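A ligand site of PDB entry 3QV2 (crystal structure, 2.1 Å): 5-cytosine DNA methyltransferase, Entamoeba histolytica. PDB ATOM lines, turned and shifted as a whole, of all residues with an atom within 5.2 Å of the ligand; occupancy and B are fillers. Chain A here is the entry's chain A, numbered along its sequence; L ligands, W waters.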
ATOM      1  N   PHE A  17      24.668 -18.582 -24.739  1.00  0.00           N
ATOM      2  CA  PHE A  17      23.829 -17.382 -24.696  1.00  0.00           C
ATOM      3  C   PHE A  17      24.670 -16.207 -24.195  1.00  0.00           C
ATOM      4  O   PHE A  17      24.249 -15.461 -23.320  1.00  0.00           O
ATOM      5  CB  PHE A  17      22.616 -17.600 -23.787  1.00  0.00           C
ATOM      6  CG  PHE A  17      21.991 -18.961 -23.929  1.00  0.00           C
ATOM      7  CD1 PHE A  17      21.124 -19.236 -24.977  1.00  0.00           C
ATOM      8  CD2 PHE A  17      22.263 -19.965 -23.024  1.00  0.00           C
ATOM      9  CE1 PHE A  17      20.555 -20.485 -25.120  1.00  0.00           C
ATOM     10  CE2 PHE A  17      21.702 -21.214 -23.148  1.00  0.00           C
ATOM     11  CZ  PHE A  17      20.840 -21.482 -24.199  1.00  0.00           C
ATOM     12  N   SER A  18      25.848 -16.050 -24.791  1.00  0.00           N
ATOM     13  CA  SER A  18      26.850 -15.107 -24.315  1.00  0.00           C
ATOM     14  C   SER A  18      26.375 -13.650 -24.220  1.00  0.00           C
ATOM     15  O   SER A  18      26.860 -12.890 -23.376  1.00  0.00           O
ATOM     16  CB  SER A  18      28.115 -15.184 -25.175  1.00  0.00           C
ATOM     17  OG  SER A  18      27.787 -15.168 -26.559  1.00  0.00           O
ATOM     18  N   GLY A  19      25.449 -13.261 -25.084  1.00  0.00           N
ATOM     19  CA  GLY A  19      24.954 -11.897 -25.087  1.00  0.00           C
ATOM     20  C   GLY A  19      26.078 -10.896 -25.278  1.00  0.00           C
ATOM     21  O   GLY A  19      26.773 -10.913 -26.298  1.00  0.00           O
ATOM     22  N   ILE A  20      26.258 -10.006 -24.299  1.00  0.00           N
ATOM     23  CA  ILE A  20      27.305  -8.994 -24.387  1.00  0.00           C
ATOM     24  C   ILE A  20      28.521  -9.346 -23.526  1.00  0.00           C
ATOM     25  O   ILE A  20      29.423  -8.533 -23.353  1.00  0.00           O
ATOM     26  CB  ILE A  20      26.787  -7.592 -23.976  1.00  0.00           C
ATOM     27  CG1 ILE A  20      26.408  -7.561 -22.498  1.00  0.00           C
ATOM     28  CG2 ILE A  20      25.599  -7.187 -24.848  1.00  0.00           C
ATOM     29  CD1 ILE A  20      25.927  -6.207 -22.024  1.00  0.00           C
ATOM     30  N   GLY A  21      28.519 -10.562 -22.985  1.00  0.00           N
ATOM     31  CA  GLY A  21      29.657 -11.054 -22.232  1.00  0.00           C
ATOM     32  C   GLY A  21      29.598 -10.771 -20.738  1.00  0.00           C
ATOM     33  O   GLY A  21      30.628 -10.561 -20.103  1.00  0.00           O
ATOM     34  N   GLY A  22      28.393 -10.779 -20.188  1.00  0.00           N
ATOM     35  CA  GLY A  22      28.211 -10.528 -18.766  1.00  0.00           C
ATOM     36  C   GLY A  22      28.854 -11.593 -17.904  1.00  0.00           C
ATOM     37  O   GLY A  22      29.500 -11.289 -16.890  1.00  0.00           O
ATOM     38  N   LEU A  23      28.680 -12.852 -18.291  1.00  0.00           N
ATOM     39  CA  LEU A  23      29.236 -13.973 -17.535  1.00  0.00           C
ATOM     40  C   LEU A  23      30.768 -13.958 -17.578  1.00  0.00           C
ATOM     41  O   LEU A  23      31.421 -14.215 -16.570  1.00  0.00           O
ATOM     42  CB  LEU A  23      28.712 -15.308 -18.067  1.00  0.00           C
ATOM     43  CG  LEU A  23      27.191 -15.448 -18.070  1.00  0.00           C
ATOM     44  CD1 LEU A  23      26.781 -16.791 -18.645  1.00  0.00           C
ATOM     45  CD2 LEU A  23      26.650 -15.290 -16.660  1.00  0.00           C
ATOM     46  N   PHE A  41      28.638 -18.492 -27.519  1.00  0.00           N
ATOM     47  CA  PHE A  41      27.633 -18.911 -28.492  1.00  0.00           C
ATOM     48  C   PHE A  41      26.402 -18.023 -28.371  1.00  0.00           C
ATOM     49  O   PHE A  41      25.824 -17.896 -27.289  1.00  0.00           O
ATOM     50  CB  PHE A  41      27.231 -20.373 -28.278  1.00  0.00           C
ATOM     51  CG  PHE A  41      28.213 -21.368 -28.827  1.00  0.00           C
ATOM     52  CD1 PHE A  41      27.979 -22.001 -30.034  1.00  0.00           C
ATOM     53  CD2 PHE A  41      29.368 -21.673 -28.136  1.00  0.00           C
ATOM     54  CE1 PHE A  41      28.872 -22.929 -30.540  1.00  0.00           C
ATOM     55  CE2 PHE A  41      30.270 -22.592 -28.634  1.00  0.00           C
ATOM     56  CZ  PHE A  41      30.023 -23.227 -29.836  1.00  0.00           C
ATOM     57  N   ASP A  42      25.998 -17.404 -29.478  1.00  0.00           N
ATOM     58  CA  ASP A  42      24.782 -16.596 -29.501  1.00  0.00           C
ATOM     59  C   ASP A  42      24.412 -16.242 -30.937  1.00  0.00           C
ATOM     60  O   ASP A  42      25.276 -16.012 -31.779  1.00  0.00           O
ATOM     61  CB  ASP A  42      24.966 -15.326 -28.658  1.00  0.00           C
ATOM     62  CG  ASP A  42      23.648 -14.710 -28.244  1.00  0.00           C
ATOM     63  OD1 ASP A  42      22.762 -14.544 -29.109  1.00  0.00           O
ATOM     64  OD2 ASP A  42      23.484 -14.408 -27.042  1.00  0.00           O
ATOM     65  N   ILE A  43      23.112 -16.205 -31.207  1.00  0.00           N
ATOM     66  CA  ILE A  43      22.603 -15.953 -32.557  1.00  0.00           C
ATOM     67  C   ILE A  43      22.227 -14.485 -32.777  1.00  0.00           C
ATOM     68  O   ILE A  43      21.897 -14.093 -33.898  1.00  0.00           O
ATOM     69  CB  ILE A  43      21.392 -16.843 -32.869  1.00  0.00           C
ATOM     70  CG1 ILE A  43      20.246 -16.529 -31.907  1.00  0.00           C
ATOM     71  CG2 ILE A  43      21.774 -18.307 -32.790  1.00  0.00           C
ATOM     72  CD1 ILE A  43      19.000 -17.369 -32.132  1.00  0.00           C
ATOM     73  N   ASN A  44      22.268 -13.697 -31.713  1.00  0.00           N
ATOM     74  CA  ASN A  44      21.918 -12.287 -31.803  1.00  0.00           C
ATOM     75  C   ASN A  44      23.058 -11.459 -32.404  1.00  0.00           C
ATOM     76  O   ASN A  44      24.075 -11.222 -31.754  1.00  0.00           O
ATOM     77  CB  ASN A  44      21.538 -11.742 -30.417  1.00  0.00           C
ATOM     78  CG  ASN A  44      20.874 -10.386 -30.485  1.00  0.00           C
ATOM     79  OD1 ASN A  44      21.528  -9.358 -30.563  1.00  0.00           O
ATOM     80  ND2 ASN A  44      19.540 -10.374 -30.452  1.00  0.00           N
ATOM     81  N   ALA A  47      24.056  -8.280 -30.354  1.00  0.00           N
ATOM     82  CA  ALA A  47      24.734  -8.669 -29.119  1.00  0.00           C
ATOM     83  C   ALA A  47      26.165  -9.113 -29.406  1.00  0.00           C
ATOM     84  O   ALA A  47      27.105  -8.707 -28.729  1.00  0.00           O
ATOM     85  CB  ALA A  47      23.966  -9.774 -28.420  1.00  0.00           C
ATOM     86  N   LYS A  62      26.150 -20.889 -34.222  1.00  0.00           N
ATOM     87  CA  LYS A  62      25.495 -22.176 -34.322  1.00  0.00           C
ATOM     88  C   LYS A  62      24.322 -22.249 -33.345  1.00  0.00           C
ATOM     89  O   LYS A  62      24.504 -22.054 -32.144  1.00  0.00           O
ATOM     90  CB  LYS A  62      26.479 -23.313 -34.046  1.00  0.00           C
ATOM     91  CG  LYS A  62      25.898 -24.705 -34.183  1.00  0.00           C
ATOM     92  CD  LYS A  62      25.368 -24.944 -35.594  1.00  0.00           C
ATOM     93  CE  LYS A  62      24.771 -26.338 -35.735  1.00  0.00           C
ATOM     94  NZ  LYS A  62      24.343 -26.624 -37.130  1.00  0.00           N
ATOM     95  N   ASN A  63      23.129 -22.507 -33.864  1.00  0.00           N
ATOM     96  CA  ASN A  63      21.923 -22.523 -33.036  1.00  0.00           C
ATOM     97  C   ASN A  63      21.992 -23.602 -31.946  1.00  0.00           C
ATOM     98  O   ASN A  63      22.250 -24.770 -32.231  1.00  0.00           O
ATOM     99  CB  ASN A  63      20.673 -22.721 -33.887  1.00  0.00           C
ATOM    100  CG  ASN A  63      19.414 -22.234 -33.195  1.00  0.00           C
ATOM    101  OD1 ASN A  63      18.937 -22.854 -32.248  1.00  0.00           O
ATOM    102  ND2 ASN A  63      18.865 -21.127 -33.676  1.00  0.00           N
ATOM    103  N   LEU A  64      21.754 -23.195 -30.708  1.00  0.00           N
ATOM    104  CA  LEU A  64      21.885 -24.085 -29.559  1.00  0.00           C
ATOM    105  C   LEU A  64      20.743 -25.086 -29.457  1.00  0.00           C
ATOM    106  O   LEU A  64      20.761 -25.980 -28.608  1.00  0.00           O
ATOM    107  CB  LEU A  64      22.013 -23.280 -28.261  1.00  0.00           C
ATOM    108  CG  LEU A  64      23.416 -22.805 -27.866  1.00  0.00           C
ATOM    109  CD1 LEU A  64      24.190 -22.348 -29.083  1.00  0.00           C
ATOM    110  CD2 LEU A  64      23.337 -21.702 -26.825  1.00  0.00           C
ATOM    111  N   ASP A  65      19.745 -24.939 -30.323  1.00  0.00           N
ATOM    112  CA  ASP A  65      18.624 -25.877 -30.348  1.00  0.00           C
ATOM    113  C   ASP A  65      19.041 -27.236 -30.871  1.00  0.00           C
ATOM    114  O   ASP A  65      18.480 -28.256 -30.486  1.00  0.00           O
ATOM    115  CB  ASP A  65      17.483 -25.339 -31.218  1.00  0.00           C
ATOM    116  CG  ASP A  65      16.791 -24.131 -30.600  1.00  0.00           C
ATOM    117  OD1 ASP A  65      16.978 -23.886 -29.391  1.00  0.00           O
ATOM    118  OD2 ASP A  65      16.059 -23.434 -31.327  1.00  0.00           O
ATOM    119  N   SER A  83      23.179 -18.038 -19.291  1.00  0.00           N
ATOM    120  CA  SER A  83      21.974 -17.398 -18.814  1.00  0.00           C
ATOM    121  C   SER A  83      20.913 -17.529 -19.908  1.00  0.00           C
ATOM    122  O   SER A  83      20.761 -16.635 -20.750  1.00  0.00           O
ATOM    123  CB  SER A  83      22.216 -15.932 -18.465  1.00  0.00           C
ATOM    124  OG  SER A  83      22.797 -15.241 -19.559  1.00  0.00           O
ATOM    125  N   PRO A  84      20.187 -18.655 -19.908  1.00  0.00           N
ATOM    126  CA  PRO A  84      19.213 -18.999 -20.937  1.00  0.00           C
ATOM    127  C   PRO A  84      18.114 -17.949 -21.061  1.00  0.00           C
ATOM    128  O   PRO A  84      17.872 -17.201 -20.114  1.00  0.00           O
ATOM    129  CB  PRO A  84      18.610 -20.310 -20.425  1.00  0.00           C
ATOM    130  CG  PRO A  84      19.655 -20.881 -19.518  1.00  0.00           C
ATOM    131  CD  PRO A  84      20.280 -19.689 -18.861  1.00  0.00           C
ATOM    132  N   PRO A  85      17.451 -17.888 -22.233  1.00  0.00           N
ATOM    133  CA  PRO A  85      16.322 -16.975 -22.418  1.00  0.00           C
ATOM    134  C   PRO A  85      15.355 -17.095 -21.251  1.00  0.00           C
ATOM    135  O   PRO A  85      15.039 -18.212 -20.828  1.00  0.00           O
ATOM    136  CB  PRO A  85      15.684 -17.484 -23.710  1.00  0.00           C
ATOM    137  CG  PRO A  85      16.822 -18.067 -24.473  1.00  0.00           C
ATOM    138  CD  PRO A  85      17.736 -18.682 -23.441  1.00  0.00           C
ATOM    139  N   SER A 107      16.647 -24.697 -26.466  1.00  0.00           N
ATOM    140  CA  SER A 107      18.102 -24.698 -26.458  1.00  0.00           C
ATOM    141  C   SER A 107      18.702 -25.196 -25.139  1.00  0.00           C
ATOM    142  O   SER A 107      19.640 -25.982 -25.140  1.00  0.00           O
ATOM    143  CB  SER A 107      18.650 -23.311 -26.812  1.00  0.00           C
ATOM    144  OG  SER A 107      18.040 -22.305 -26.018  1.00  0.00           O
ATOM    145  N   PHE A 285      30.323  -3.804 -15.441  1.00  0.00           N
ATOM    146  CA  PHE A 285      31.253  -4.095 -16.525  1.00  0.00           C
ATOM    147  C   PHE A 285      32.499  -3.239 -16.375  1.00  0.00           C
ATOM    148  O   PHE A 285      32.453  -2.179 -15.742  1.00  0.00           O
ATOM    149  CB  PHE A 285      30.588  -3.858 -17.892  1.00  0.00           C
ATOM    150  CG  PHE A 285      29.511  -4.856 -18.220  1.00  0.00           C
ATOM    151  CD1 PHE A 285      29.757  -5.897 -19.101  1.00  0.00           C
ATOM    152  CD2 PHE A 285      28.254  -4.742 -17.652  1.00  0.00           C
ATOM    153  CE1 PHE A 285      28.762  -6.808 -19.408  1.00  0.00           C
ATOM    154  CE2 PHE A 285      27.255  -5.647 -17.948  1.00  0.00           C
ATOM    155  CZ  PHE A 285      27.514  -6.687 -18.833  1.00  0.00           C
ATOM    156  N   CYS A 304      20.200  -4.717 -25.091  1.00  0.00           N
ATOM    157  CA  CYS A 304      21.229  -5.660 -24.697  1.00  0.00           C
ATOM    158  C   CYS A 304      21.536  -5.552 -23.211  1.00  0.00           C
ATOM    159  O   CYS A 304      21.597  -6.559 -22.504  1.00  0.00           O
ATOM    160  CB  CYS A 304      22.506  -5.424 -25.513  1.00  0.00           C
ATOM    161  SG  CYS A 304      22.351  -5.794 -27.277  1.00  0.00           S
ATOM    162  N   ASN A 307      19.000  -6.948 -20.922  1.00  0.00           N
ATOM    163  CA  ASN A 307      19.002  -8.406 -20.925  1.00  0.00           C
ATOM    164  C   ASN A 307      20.270  -9.010 -20.304  1.00  0.00           C
ATOM    165  O   ASN A 307      20.409 -10.228 -20.234  1.00  0.00           O
ATOM    166  CB  ASN A 307      18.820  -8.936 -22.346  1.00  0.00           C
ATOM    167  CG  ASN A 307      17.411  -8.761 -22.864  1.00  0.00           C
ATOM    168  OD1 ASN A 307      16.440  -8.886 -22.112  1.00  0.00           O
ATOM    169  ND2 ASN A 307      17.284  -8.458 -24.156  1.00  0.00           N
ATOM    170  N   SER A 308      21.176  -8.154 -19.845  1.00  0.00           N
ATOM    171  CA  SER A 308      22.452  -8.620 -19.304  1.00  0.00           C
ATOM    172  C   SER A 308      22.328  -9.060 -17.852  1.00  0.00           C
ATOM    173  O   SER A 308      21.287  -9.582 -17.442  1.00  0.00           O
ATOM    174  CB  SER A 308      23.528  -7.540 -19.436  1.00  0.00           C
ATOM    175  OG  SER A 308      23.258  -6.438 -18.579  1.00  0.00           O
ATOM    176  N   VAL A 309      23.380  -8.837 -17.075  1.00  0.00           N
ATOM    177  CA  VAL A 309      23.436  -9.321 -15.701  1.00  0.00           C
ATOM    178  C   VAL A 309      24.135  -8.334 -14.770  1.00  0.00           C
ATOM    179  O   VAL A 309      24.622  -7.286 -15.202  1.00  0.00           O
ATOM    180  CB  VAL A 309      24.206 -10.660 -15.609  1.00  0.00           C
ATOM    181  CG1 VAL A 309      23.500 -11.743 -16.408  1.00  0.00           C
ATOM    182  CG2 VAL A 309      25.635 -10.480 -16.097  1.00  0.00           C
HETATM  183  N1  LIG L   1      23.931 -12.978 -20.113  1.00  0.00           N
HETATM  184  C1  LIG L   1      24.152 -12.341 -21.391  1.00  0.00           C
HETATM  185  C2  LIG L   1      22.846 -12.248 -22.183  1.00  0.00           C
HETATM  186  C3  LIG L   1      21.782 -13.294 -21.949  1.00  0.00           C
HETATM  187  S1  LIG L   1      20.222 -13.090 -22.839  1.00  0.00           S
HETATM  188  C4  LIG L   1      24.754 -10.977 -21.166  1.00  0.00           C
HETATM  189  O1  LIG L   1      24.553 -10.059 -22.011  1.00  0.00           O
HETATM  190  O2  LIG L   1      25.462 -10.753 -20.132  1.00  0.00           O
HETATM  191  C5  LIG L   1      19.879 -14.573 -23.759  1.00  0.00           C
HETATM  192  C6  LIG L   1      20.596 -14.788 -25.041  1.00  0.00           C
HETATM  193  O3  LIG L   1      20.390 -16.093 -25.448  1.00  0.00           O
HETATM  194  C7  LIG L   1      20.033 -13.910 -26.070  1.00  0.00           C
HETATM  195  O4  LIG L   1      20.960 -12.953 -26.432  1.00  0.00           O
HETATM  196  C8  LIG L   1      19.697 -14.740 -27.204  1.00  0.00           C
HETATM  197  O5  LIG L   1      20.231 -14.188 -28.363  1.00  0.00           O
HETATM  198  C9  LIG L   1      20.318 -16.035 -26.908  1.00  0.00           C
HETATM  199  N2  LIG L   1      19.609 -17.116 -27.534  1.00  0.00           N
HETATM  200  C10 LIG L   1      18.307 -17.398 -27.542  1.00  0.00           C
HETATM  201  N3  LIG L   1      18.143 -18.520 -28.267  1.00  0.00           N
HETATM  202  C11 LIG L   1      19.356 -18.933 -28.697  1.00  0.00           C
HETATM  203  C12 LIG L   1      19.787 -20.014 -29.465  1.00  0.00           C
HETATM  204  N4  LIG L   1      18.833 -20.980 -29.979  1.00  0.00           N
HETATM  205  N5  LIG L   1      21.095 -20.138 -29.720  1.00  0.00           N
HETATM  206  C13 LIG L   1      21.999 -19.253 -29.261  1.00  0.00           C
HETATM  207  N6  LIG L   1      21.608 -18.210 -28.518  1.00  0.00           N
HETATM  208  C14 LIG L   1      20.305 -18.030 -28.233  1.00  0.00           C
HETATM  209  O   HOH W   1      17.885 -12.514 -20.427  1.00  0.00           O
HETATM  210  O   HOH W   2      24.925 -19.604 -30.893  1.00  0.00           O
HETATM  211  O   HOH W   3      21.052 -12.543 -18.553  1.00  0.00           O
HETATM  212  O   HOH W   4      25.018 -15.615 -20.850  1.00  0.00           O
HETATM  213  O   HOH W   5      16.384 -20.770 -31.891  1.00  0.00           O
HETATM  214  O   HOH W   6      18.444 -13.473 -30.404  1.00  0.00           O
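N1 of the ligand sits at hydrogen-bond distance from OG of Ser 83 (2.6 Å). OD1 of Asp 42 sits at hydrogen-bond distance from O5 of the ligand (2.7 Å). N of Ile 20 is in hydrogen-bond range of O1 of the ligand. An oxygen (O2) of the ligand lies within hydrogen-bond range of the backbone NH (N) of Gly 22 (2.9 Å). The side-chain amide oxygen of Asn 63 is in hydrogen-bond range of a nitrogen (N4) of the ligand. A nitrogen (N5) of the ligand is in hydrogen-bond range of the backbone NH of Leu 64 (3.3 Å). OD1 of Asp 65 is in hydrogen-bond range of N4 of the ligand, at 3.5 Å.
The side-chain carboxylate (OD1) of Asp 42 is in hydrogen-bond range of the backbone NH (N) of Asn 44 (2.8 Å). OD2 of Asp 42 is in hydrogen-bond range of N of Gly 19 (3.0 Å). The side-chain amide oxygen of Asn 63 is in hydrogen-bond range of the backbone NH of Asp 65 (3.0 Å). The backbone NH of Phe 17 is in hydrogen-bond range of the backbone carbonyl oxygen of Phe 41, 2.9 Å away. O of Phe 41 lies within hydrogen-bond range of N of Ser 18, 3.1 Å away. The backbone NH of Ala 47 lies within hydrogen-bond range of the side-chain amide oxygen of Asn 44, at 2.8 Å. The side-chain carboxylate (OD1) of Asp 65 lies within hydrogen-bond range of the backbone NH (N) of Ser 107 (3.1 Å).
Residues that only touch the ligand: Phe 17, Ser 18, Asn 44, Pro 85, Gly 19, Ile 43, Ser 308, Asn 307, Val 309 and Ser 107. Hydrophobic or aromatic side chains that line the ligand: Phe 17, Ile 20, Ile 43, Leu 64, Pro 85 and Val 309. Within 4 Å of the ligand: Phe 17, Ser 18, Gly 19, Ile 20, Gly 22, Asp 42, Ile 43, Asn 44, Asn 63, Leu 64, Asp 65, Ser 83, Pro 85, Ser 107, Asn 307, Ser 308 and Val 309. The nearest printed residue that does not touch the ligand is Gly 21 (4.1 Å).
Water W6 bridges an oxygen (O5) of the ligand (2.8 Å) and the side-chain amide nitrogen (ND2) of Asn 44 (3.3 Å). Water W4 lies within hydrogen-bond range of the backbone carbonyl oxygen (O) of Phe 17, the side-chain hydroxyl (OG) of Ser 83 and a nitrogen (N1) of the ligand. Water W5 lies within hydrogen-bond range of the side-chain carboxylate of Asp 65 (2.7 Å), the side-chain amide nitrogen of Asn 63 (3.1 Å) and a nitrogen (N4) of the ligand (3.1 Å). Water W3 lies within hydrogen-bond range of the backbone carbonyl oxygen (O) of Asn 307 (2.9 Å), the backbone carbonyl oxygen (O) of Ser 308 (3.2 Å), a nitrogen (N1) of the ligand (3.3 Å) and the side-chain hydroxyl (OG) of Ser 83 (3.4 Å). Water W2 lies within hydrogen-bond range of O of Lys 62 and N of Asp 42. Water W1 bridges a sulfur (S1) of the ligand and the backbone carbonyl oxygen (O) of Asn 307.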
